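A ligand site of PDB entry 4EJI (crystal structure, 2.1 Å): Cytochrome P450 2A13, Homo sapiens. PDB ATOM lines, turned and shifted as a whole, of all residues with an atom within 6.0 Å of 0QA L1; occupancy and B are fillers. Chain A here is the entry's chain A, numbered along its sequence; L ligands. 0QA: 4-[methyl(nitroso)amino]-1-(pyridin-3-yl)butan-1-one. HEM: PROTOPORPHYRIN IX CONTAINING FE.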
ATOM      1  N   PHE A  85      -7.125  -6.061  19.184  1.00  0.00           N
ATOM      2  CA  PHE A  85      -7.302  -6.552  20.540  1.00  0.00           C
ATOM      3  C   PHE A  85      -6.054  -6.806  21.365  1.00  0.00           C
ATOM      4  O   PHE A  85      -6.184  -6.758  22.602  1.00  0.00           O
ATOM      5  CB  PHE A  85      -8.168  -7.818  20.565  1.00  0.00           C
ATOM      6  CG  PHE A  85      -9.519  -7.636  19.934  1.00  0.00           C
ATOM      7  CD1 PHE A  85      -9.858  -8.331  18.788  1.00  0.00           C
ATOM      8  CD2 PHE A  85     -10.443  -6.760  20.471  1.00  0.00           C
ATOM      9  CE1 PHE A  85     -11.155  -8.204  18.194  1.00  0.00           C
ATOM     10  CE2 PHE A  85     -11.727  -6.577  19.894  1.00  0.00           C
ATOM     11  CZ  PHE A  85     -12.102  -7.314  18.746  1.00  0.00           C
ATOM     12  N   PHE A  89      -5.283  -7.317  25.569  1.00  0.00           N
ATOM     13  CA  PHE A  89      -5.152  -8.678  26.111  1.00  0.00           C
ATOM     14  C   PHE A  89      -3.712  -9.109  26.359  1.00  0.00           C
ATOM     15  O   PHE A  89      -3.440  -9.788  27.345  1.00  0.00           O
ATOM     16  CB  PHE A  89      -5.884  -9.756  25.255  1.00  0.00           C
ATOM     17  CG  PHE A  89      -7.391  -9.614  25.278  1.00  0.00           C
ATOM     18  CD1 PHE A  89      -8.054  -8.775  24.356  1.00  0.00           C
ATOM     19  CD2 PHE A  89      -8.153 -10.264  26.257  1.00  0.00           C
ATOM     20  CE1 PHE A  89      -9.425  -8.588  24.392  1.00  0.00           C
ATOM     21  CE2 PHE A  89      -9.569 -10.083  26.296  1.00  0.00           C
ATOM     22  CZ  PHE A  89     -10.202  -9.242  25.345  1.00  0.00           C
ATOM     23  N   ALA A  95      -9.096 -16.808  24.973  1.00  0.00           N
ATOM     24  CA  ALA A  95      -9.193 -16.608  23.520  1.00  0.00           C
ATOM     25  C   ALA A  95      -7.879 -16.098  22.942  1.00  0.00           C
ATOM     26  O   ALA A  95      -7.592 -16.310  21.792  1.00  0.00           O
ATOM     27  CB  ALA A  95     -10.308 -15.620  23.158  1.00  0.00           C
ATOM     28  N   PHE A  96      -7.110 -15.421  23.754  1.00  0.00           N
ATOM     29  CA  PHE A  96      -5.880 -14.805  23.196  1.00  0.00           C
ATOM     30  C   PHE A  96      -4.611 -15.472  23.608  1.00  0.00           C
ATOM     31  O   PHE A  96      -3.575 -14.964  23.308  1.00  0.00           O
ATOM     32  CB  PHE A  96      -5.839 -13.321  23.553  1.00  0.00           C
ATOM     33  CG  PHE A  96      -6.836 -12.567  22.801  1.00  0.00           C
ATOM     34  CD1 PHE A  96      -8.127 -12.455  23.268  1.00  0.00           C
ATOM     35  CD2 PHE A  96      -6.514 -12.059  21.563  1.00  0.00           C
ATOM     36  CE1 PHE A  96      -9.075 -11.814  22.560  1.00  0.00           C
ATOM     37  CE2 PHE A  96      -7.499 -11.424  20.831  1.00  0.00           C
ATOM     38  CZ  PHE A  96      -8.781 -11.308  21.351  1.00  0.00           C
ATOM     39  N   SER A 186     -17.141  -1.999  19.163  1.00  0.00           N
ATOM     40  CA  SER A 186     -15.820  -2.601  18.959  1.00  0.00           C
ATOM     41  C   SER A 186     -15.894  -3.787  18.021  1.00  0.00           C
ATOM     42  O   SER A 186     -15.061  -3.937  17.150  1.00  0.00           O
ATOM     43  CB  SER A 186     -15.100  -2.931  20.240  1.00  0.00           C
ATOM     44  OG  SER A 186     -15.869  -3.757  21.066  1.00  0.00           O
ATOM     45  N   PHE A 187     -16.917  -4.626  18.182  1.00  0.00           N
ATOM     46  CA  PHE A 187     -17.182  -5.663  17.228  1.00  0.00           C
ATOM     47  C   PHE A 187     -17.291  -5.193  15.761  1.00  0.00           C
ATOM     48  O   PHE A 187     -16.666  -5.780  14.887  1.00  0.00           O
ATOM     49  CB  PHE A 187     -18.454  -6.351  17.644  1.00  0.00           C
ATOM     50  CG  PHE A 187     -18.718  -7.585  16.919  1.00  0.00           C
ATOM     51  CD1 PHE A 187     -17.985  -8.721  17.176  1.00  0.00           C
ATOM     52  CD2 PHE A 187     -19.755  -7.651  16.022  1.00  0.00           C
ATOM     53  CE1 PHE A 187     -18.292  -9.934  16.528  1.00  0.00           C
ATOM     54  CE2 PHE A 187     -20.055  -8.823  15.353  1.00  0.00           C
ATOM     55  CZ  PHE A 187     -19.317  -9.977  15.582  1.00  0.00           C
ATOM     56  N   LEU A 219     -13.327  -1.012  24.475  1.00  0.00           N
ATOM     57  CA  LEU A 219     -12.663  -2.179  24.978  1.00  0.00           C
ATOM     58  C   LEU A 219     -12.108  -1.935  26.398  1.00  0.00           C
ATOM     59  O   LEU A 219     -12.325  -2.788  27.251  1.00  0.00           O
ATOM     60  CB  LEU A 219     -11.568  -2.643  24.004  1.00  0.00           C
ATOM     61  CG  LEU A 219     -12.141  -3.302  22.746  1.00  0.00           C
ATOM     62  CD1 LEU A 219     -11.108  -3.279  21.502  1.00  0.00           C
ATOM     63  CD2 LEU A 219     -12.584  -4.691  23.183  1.00  0.00           C
ATOM     64  N   MET A 271      -9.320 -11.099  31.788  1.00  0.00           N
ATOM     65  CA  MET A 271      -9.343 -11.377  30.354  1.00  0.00           C
ATOM     66  C   MET A 271     -10.254 -12.525  29.847  1.00  0.00           C
ATOM     67  O   MET A 271     -10.964 -12.366  28.842  1.00  0.00           O
ATOM     68  CB  MET A 271      -7.920 -11.465  29.768  1.00  0.00           C
ATOM     69  CG  MET A 271      -7.081 -10.201  30.043  1.00  0.00           C
ATOM     70  SD  MET A 271      -7.972  -8.641  29.571  1.00  0.00           S
ATOM     71  CE  MET A 271      -6.608  -7.498  30.035  1.00  0.00           C
ATOM     72  N   LEU A 274     -13.888 -11.255  30.376  1.00  0.00           N
ATOM     73  CA  LEU A 274     -14.085 -10.390  29.253  1.00  0.00           C
ATOM     74  C   LEU A 274     -14.385 -11.210  27.988  1.00  0.00           C
ATOM     75  O   LEU A 274     -15.377 -10.897  27.309  1.00  0.00           O
ATOM     76  CB  LEU A 274     -12.940  -9.403  29.034  1.00  0.00           C
ATOM     77  CG  LEU A 274     -13.153  -8.373  27.906  1.00  0.00           C
ATOM     78  CD1 LEU A 274     -14.547  -7.681  27.936  1.00  0.00           C
ATOM     79  CD2 LEU A 274     -12.064  -7.338  27.993  1.00  0.00           C
ATOM     80  N   ASN A 275     -13.600 -12.277  27.709  1.00  0.00           N
ATOM     81  CA  ASN A 275     -13.809 -13.076  26.496  1.00  0.00           C
ATOM     82  C   ASN A 275     -15.229 -13.692  26.478  1.00  0.00           C
ATOM     83  O   ASN A 275     -15.913 -13.658  25.445  1.00  0.00           O
ATOM     84  CB  ASN A 275     -12.819 -14.240  26.389  1.00  0.00           C
ATOM     85  CG  ASN A 275     -11.398 -13.811  26.154  1.00  0.00           C
ATOM     86  OD1 ASN A 275     -11.205 -12.768  25.547  1.00  0.00           O
ATOM     87  ND2 ASN A 275     -10.381 -14.573  26.662  1.00  0.00           N
ATOM     88  N   LEU A 276     -15.606 -14.347  27.595  1.00  0.00           N
ATOM     89  CA  LEU A 276     -16.918 -14.975  27.678  1.00  0.00           C
ATOM     90  C   LEU A 276     -18.105 -13.994  27.568  1.00  0.00           C
ATOM     91  O   LEU A 276     -19.055 -14.275  26.872  1.00  0.00           O
ATOM     92  CB  LEU A 276     -17.081 -15.856  28.926  1.00  0.00           C
ATOM     93  CG  LEU A 276     -15.982 -16.863  29.211  1.00  0.00           C
ATOM     94  CD1 LEU A 276     -16.326 -17.574  30.497  1.00  0.00           C
ATOM     95  CD2 LEU A 276     -15.795 -17.783  28.014  1.00  0.00           C
ATOM     96  N   PHE A 278     -18.096 -10.937  26.230  1.00  0.00           N
ATOM     97  CA  PHE A 278     -18.105 -10.419  24.862  1.00  0.00           C
ATOM     98  C   PHE A 278     -18.527 -11.502  23.845  1.00  0.00           C
ATOM     99  O   PHE A 278     -19.454 -11.312  23.083  1.00  0.00           O
ATOM    100  CB  PHE A 278     -16.747  -9.798  24.520  1.00  0.00           C
ATOM    101  CG  PHE A 278     -16.741  -8.981  23.247  1.00  0.00           C
ATOM    102  CD1 PHE A 278     -16.462  -7.628  23.301  1.00  0.00           C
ATOM    103  CD2 PHE A 278     -16.910  -9.575  21.997  1.00  0.00           C
ATOM    104  CE1 PHE A 278     -16.439  -6.840  22.157  1.00  0.00           C
ATOM    105  CE2 PHE A 278     -16.849  -8.751  20.811  1.00  0.00           C
ATOM    106  CZ  PHE A 278     -16.643  -7.384  20.942  1.00  0.00           C
ATOM    107  N   ALA A 279     -17.807 -12.600  23.799  1.00  0.00           N
ATOM    108  CA  ALA A 279     -18.110 -13.655  22.850  1.00  0.00           C
ATOM    109  C   ALA A 279     -19.564 -14.142  23.018  1.00  0.00           C
ATOM    110  O   ALA A 279     -20.293 -14.330  22.035  1.00  0.00           O
ATOM    111  CB  ALA A 279     -17.113 -14.825  23.007  1.00  0.00           C
ATOM    112  N   GLY A 280     -19.997 -14.297  24.274  1.00  0.00           N
ATOM    113  CA  GLY A 280     -21.401 -14.684  24.630  1.00  0.00           C
ATOM    114  C   GLY A 280     -22.533 -13.712  24.323  1.00  0.00           C
ATOM    115  O   GLY A 280     -23.719 -14.078  24.414  1.00  0.00           O
ATOM    116  N   THR A 283     -21.989 -12.341  19.032  1.00  0.00           N
ATOM    117  CA  THR A 283     -22.150 -13.194  17.832  1.00  0.00           C
ATOM    118  C   THR A 283     -23.579 -13.695  17.701  1.00  0.00           C
ATOM    119  O   THR A 283     -24.172 -13.615  16.625  1.00  0.00           O
ATOM    120  CB  THR A 283     -21.142 -14.390  17.774  1.00  0.00           C
ATOM    121  OG1 THR A 283     -20.775 -14.800  19.103  1.00  0.00           O
ATOM    122  CG2 THR A 283     -19.879 -14.008  17.023  1.00  0.00           C
ATOM    123  N   LEU A 344     -17.945 -14.583  11.499  1.00  0.00           N
ATOM    124  CA  LEU A 344     -16.500 -14.400  11.682  1.00  0.00           C
ATOM    125  C   LEU A 344     -15.744 -14.891  10.409  1.00  0.00           C
ATOM    126  O   LEU A 344     -15.297 -16.033  10.387  1.00  0.00           O
ATOM    127  CB  LEU A 344     -16.068 -15.155  12.930  1.00  0.00           C
ATOM    128  CG  LEU A 344     -16.478 -14.623  14.307  1.00  0.00           C
ATOM    129  CD1 LEU A 344     -15.490 -15.127  15.440  1.00  0.00           C
ATOM    130  CD2 LEU A 344     -16.550 -13.142  14.290  1.00  0.00           C
ATOM    131  N   LEU A 348     -10.749 -16.551  14.069  1.00  0.00           N
ATOM    132  CA  LEU A 348      -9.692 -15.901  14.810  1.00  0.00           C
ATOM    133  C   LEU A 348      -8.374 -16.387  14.143  1.00  0.00           C
ATOM    134  O   LEU A 348      -8.297 -17.517  13.638  1.00  0.00           O
ATOM    135  CB  LEU A 348      -9.808 -16.288  16.305  1.00  0.00           C
ATOM    136  CG  LEU A 348     -10.347 -15.428  17.461  1.00  0.00           C
ATOM    137  CD1 LEU A 348     -11.423 -14.387  17.109  1.00  0.00           C
ATOM    138  CD2 LEU A 348     -10.734 -16.273  18.738  1.00  0.00           C
ATOM    139  N   CYS A 417     -14.663 -23.082  18.631  1.00  0.00           N
ATOM    140  CA  CYS A 417     -15.480 -22.318  19.578  1.00  0.00           C
ATOM    141  C   CYS A 417     -16.162 -23.244  20.633  1.00  0.00           C
ATOM    142  O   CYS A 417     -17.057 -23.979  20.300  1.00  0.00           O
ATOM    143  CB  CYS A 417     -16.527 -21.476  18.841  1.00  0.00           C
ATOM    144  SG  CYS A 417     -17.653 -20.650  19.955  1.00  0.00           S
HETATM  145  O2  0QA L   1     -12.970 -10.424  24.509  1.00  0.00           O
HETATM  146  N3  0QA L   1     -12.923 -10.870  23.380  1.00  0.00           N
HETATM  147  N2  0QA L   1     -13.155 -10.032  22.359  1.00  0.00           N
HETATM  148  C10 0QA L   1     -12.893  -8.600  22.635  1.00  0.00           C
HETATM  149  C9  0QA L   1     -12.315 -10.462  21.224  1.00  0.00           C
HETATM  150  C8  0QA L   1     -12.529 -11.909  20.786  1.00  0.00           C
HETATM  151  C7  0QA L   1     -13.891 -12.535  21.112  1.00  0.00           C
HETATM  152  C6  0QA L   1     -13.962 -13.910  20.461  1.00  0.00           C
HETATM  153  O1  0QA L   1     -12.997 -14.639  20.371  1.00  0.00           O
HETATM  154  C5  0QA L   1     -15.227 -14.454  19.957  1.00  0.00           C
HETATM  155  C1  0QA L   1     -16.183 -13.629  19.398  1.00  0.00           C
HETATM  156  C2  0QA L   1     -17.354 -14.289  18.992  1.00  0.00           C
HETATM  157  C3  0QA L   1     -17.493 -15.661  19.157  1.00  0.00           C
HETATM  158  N1  0QA L   1     -16.572 -16.411  19.742  1.00  0.00           N
HETATM  159  C4  0QA L   1     -15.454 -15.808  20.112  1.00  0.00           C
HETATM  160  CHA HEM L   2     -13.675 -18.847  19.388  1.00  0.00           C
HETATM  161  CHB HEM L   2     -17.427 -18.556  16.384  1.00  0.00           C
HETATM  162  CHC HEM L   2     -20.427 -18.065  20.201  1.00  0.00           C
HETATM  163  CHD HEM L   2     -16.628 -18.305  23.238  1.00  0.00           C
HETATM  164  C1A HEM L   2     -14.417 -18.774  18.229  1.00  0.00           C
HETATM  165  C2A HEM L   2     -13.898 -18.932  16.876  1.00  0.00           C
HETATM  166  C3A HEM L   2     -14.946 -18.875  16.040  1.00  0.00           C
HETATM  167  C4A HEM L   2     -16.143 -18.690  16.858  1.00  0.00           C
HETATM  168  CMA HEM L   2     -15.007 -18.930  14.519  1.00  0.00           C
HETATM  169  CAA HEM L   2     -12.389 -19.114  16.562  1.00  0.00           C
HETATM  170  CBA HEM L   2     -11.918 -20.513  16.937  1.00  0.00           C
HETATM  171  CGA HEM L   2     -10.520 -20.633  16.381  1.00  0.00           C
HETATM  172  O1A HEM L   2     -10.392 -21.203  15.282  1.00  0.00           O
HETATM  173  O2A HEM L   2      -9.562 -20.100  16.981  1.00  0.00           O
HETATM  174  C1B HEM L   2     -18.584 -18.317  17.110  1.00  0.00           C
HETATM  175  C2B HEM L   2     -19.926 -18.045  16.575  1.00  0.00           C
HETATM  176  C3B HEM L   2     -20.718 -17.906  17.675  1.00  0.00           C
HETATM  177  C4B HEM L   2     -19.952 -18.136  18.886  1.00  0.00           C
HETATM  178  CMB HEM L   2     -20.283 -17.854  15.069  1.00  0.00           C
HETATM  179  CAB HEM L   2     -22.204 -17.570  17.759  1.00  0.00           C
HETATM  180  CBB HEM L   2     -23.026 -17.622  16.720  1.00  0.00           C
HETATM  181  C1C HEM L   2     -19.673 -18.088  21.347  1.00  0.00           C
HETATM  182  C2C HEM L   2     -20.143 -18.030  22.715  1.00  0.00           C
HETATM  183  C3C HEM L   2     -19.110 -18.079  23.546  1.00  0.00           C
HETATM  184  C4C HEM L   2     -17.916 -18.223  22.748  1.00  0.00           C
HETATM  185  CMC HEM L   2     -21.595 -17.917  23.132  1.00  0.00           C
HETATM  186  CAC HEM L   2     -19.169 -18.025  25.087  1.00  0.00           C
HETATM  187  CBC HEM L   2     -19.053 -19.171  25.739  1.00  0.00           C
HETATM  188  C1D HEM L   2     -15.496 -18.494  22.504  1.00  0.00           C
HETATM  189  C2D HEM L   2     -14.162 -18.574  23.079  1.00  0.00           C
HETATM  190  C3D HEM L   2     -13.235 -18.753  21.898  1.00  0.00           C
HETATM  191  C4D HEM L   2     -14.090 -18.738  20.710  1.00  0.00           C
HETATM  192  CMD HEM L   2     -13.788 -18.493  24.593  1.00  0.00           C
HETATM  193  CAD HEM L   2     -11.730 -18.938  21.970  1.00  0.00           C
HETATM  194  CBD HEM L   2     -11.422 -20.436  22.099  1.00  0.00           C
HETATM  195  CGD HEM L   2      -9.911 -20.678  22.086  1.00  0.00           C
HETATM  196  O1D HEM L   2      -9.448 -21.844  22.236  1.00  0.00           O
HETATM  197  O2D HEM L   2      -9.129 -19.700  21.897  1.00  0.00           O
HETATM  198  NA  HEM L   2     -15.783 -18.644  18.179  1.00  0.00           N
HETATM  199  NB  HEM L   2     -18.675 -18.348  18.497  1.00  0.00           N
HETATM  200  NC  HEM L   2     -18.312 -18.200  21.425  1.00  0.00           N
HETATM  201  ND  HEM L   2     -15.392 -18.576  21.115  1.00  0.00           N
HETATM  202 FE   HEM L   2     -17.034 -18.412  19.794  1.00  0.00          FE
HETATM  203  O2  0QA L   3     -14.922 -10.749  17.832  1.00  0.00           O
HETATM  204  N3  0QA L   3     -14.175 -11.238  17.002  1.00  0.00           N
HETATM  205  N2  0QA L   3     -13.947 -10.716  15.790  1.00  0.00           N
HETATM  206  C10 0QA L   3     -14.631  -9.405  15.705  1.00  0.00           C
HETATM  207  C9  0QA L   3     -12.492 -10.552  15.699  1.00  0.00           C
HETATM  208  C8  0QA L   3     -11.857 -11.196  14.492  1.00  0.00           C
HETATM  209  C7  0QA L   3     -10.461 -11.589  14.882  1.00  0.00           C
HETATM  210  C6  0QA L   3      -9.473 -10.624  14.271  1.00  0.00           C
HETATM  211  O1  0QA L   3      -9.402  -9.477  14.662  1.00  0.00           O
HETATM  212  C5  0QA L   3      -8.524 -11.124  13.217  1.00  0.00           C
HETATM  213  C1  0QA L   3      -7.352 -10.396  12.927  1.00  0.00           C
HETATM  214  C2  0QA L   3      -6.482 -10.898  11.962  1.00  0.00           C
HETATM  215  C3  0QA L   3      -6.791 -12.094  11.328  1.00  0.00           C
HETATM  216  N1  0QA L   3      -7.892 -12.791  11.642  1.00  0.00           N
HETATM  217  C4  0QA L   3      -8.755 -12.330  12.573  1.00  0.00           C
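A nitrogen (N1) of 0QA L1 binds an iron atom (FE) of HEM L2, 2.1 Å away.
Phe 85 touches 0QA L1 (CE2 to C10, 3.6 Å). Phe 89 touches 0QA L1. Ala 95 touches 0QA L1 (CB to O1, 3.995 Å). CZ of Phe 96 touches C9 of 0QA L1, 3.6 Å away. Leu 219 touches 0QA L1. Leu 274 touches 0QA L1. CD1 of Phe 278 touches C10 of 0QA L1, at 3.8 Å. Ala 279 touches 0QA L1. Thr 283 touches 0QA L1. CD2 of Leu 348 touches O1 of 0QA L1, 3.2 Å away. Hydrophobic or aromatic side chains that line 0QA L1: Phe 85, Phe 89, Ala 95, Phe 96, Leu 219, Leu 274, Phe 278, Ala 279 and Leu 348.
ND2 of Asn 275 sits close to N of Ala 95 (3.1 Å). O of Met 271 lies close to ND2 of Asn 275, 3.2 Å away. The side-chain hydroxyl (OG1) of Thr 283 sits at hydrogen-bond distance from the backbone carbonyl oxygen (O) of Ala 279, 3.0 Å away.
The side-chain amide oxygen (OD1) of Asn 275 lies close to an oxygen (O2) of 0QA L1 (3.1 Å). FE of HEM L2 is bound by SG of Cys 417, 2.3 Å away.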
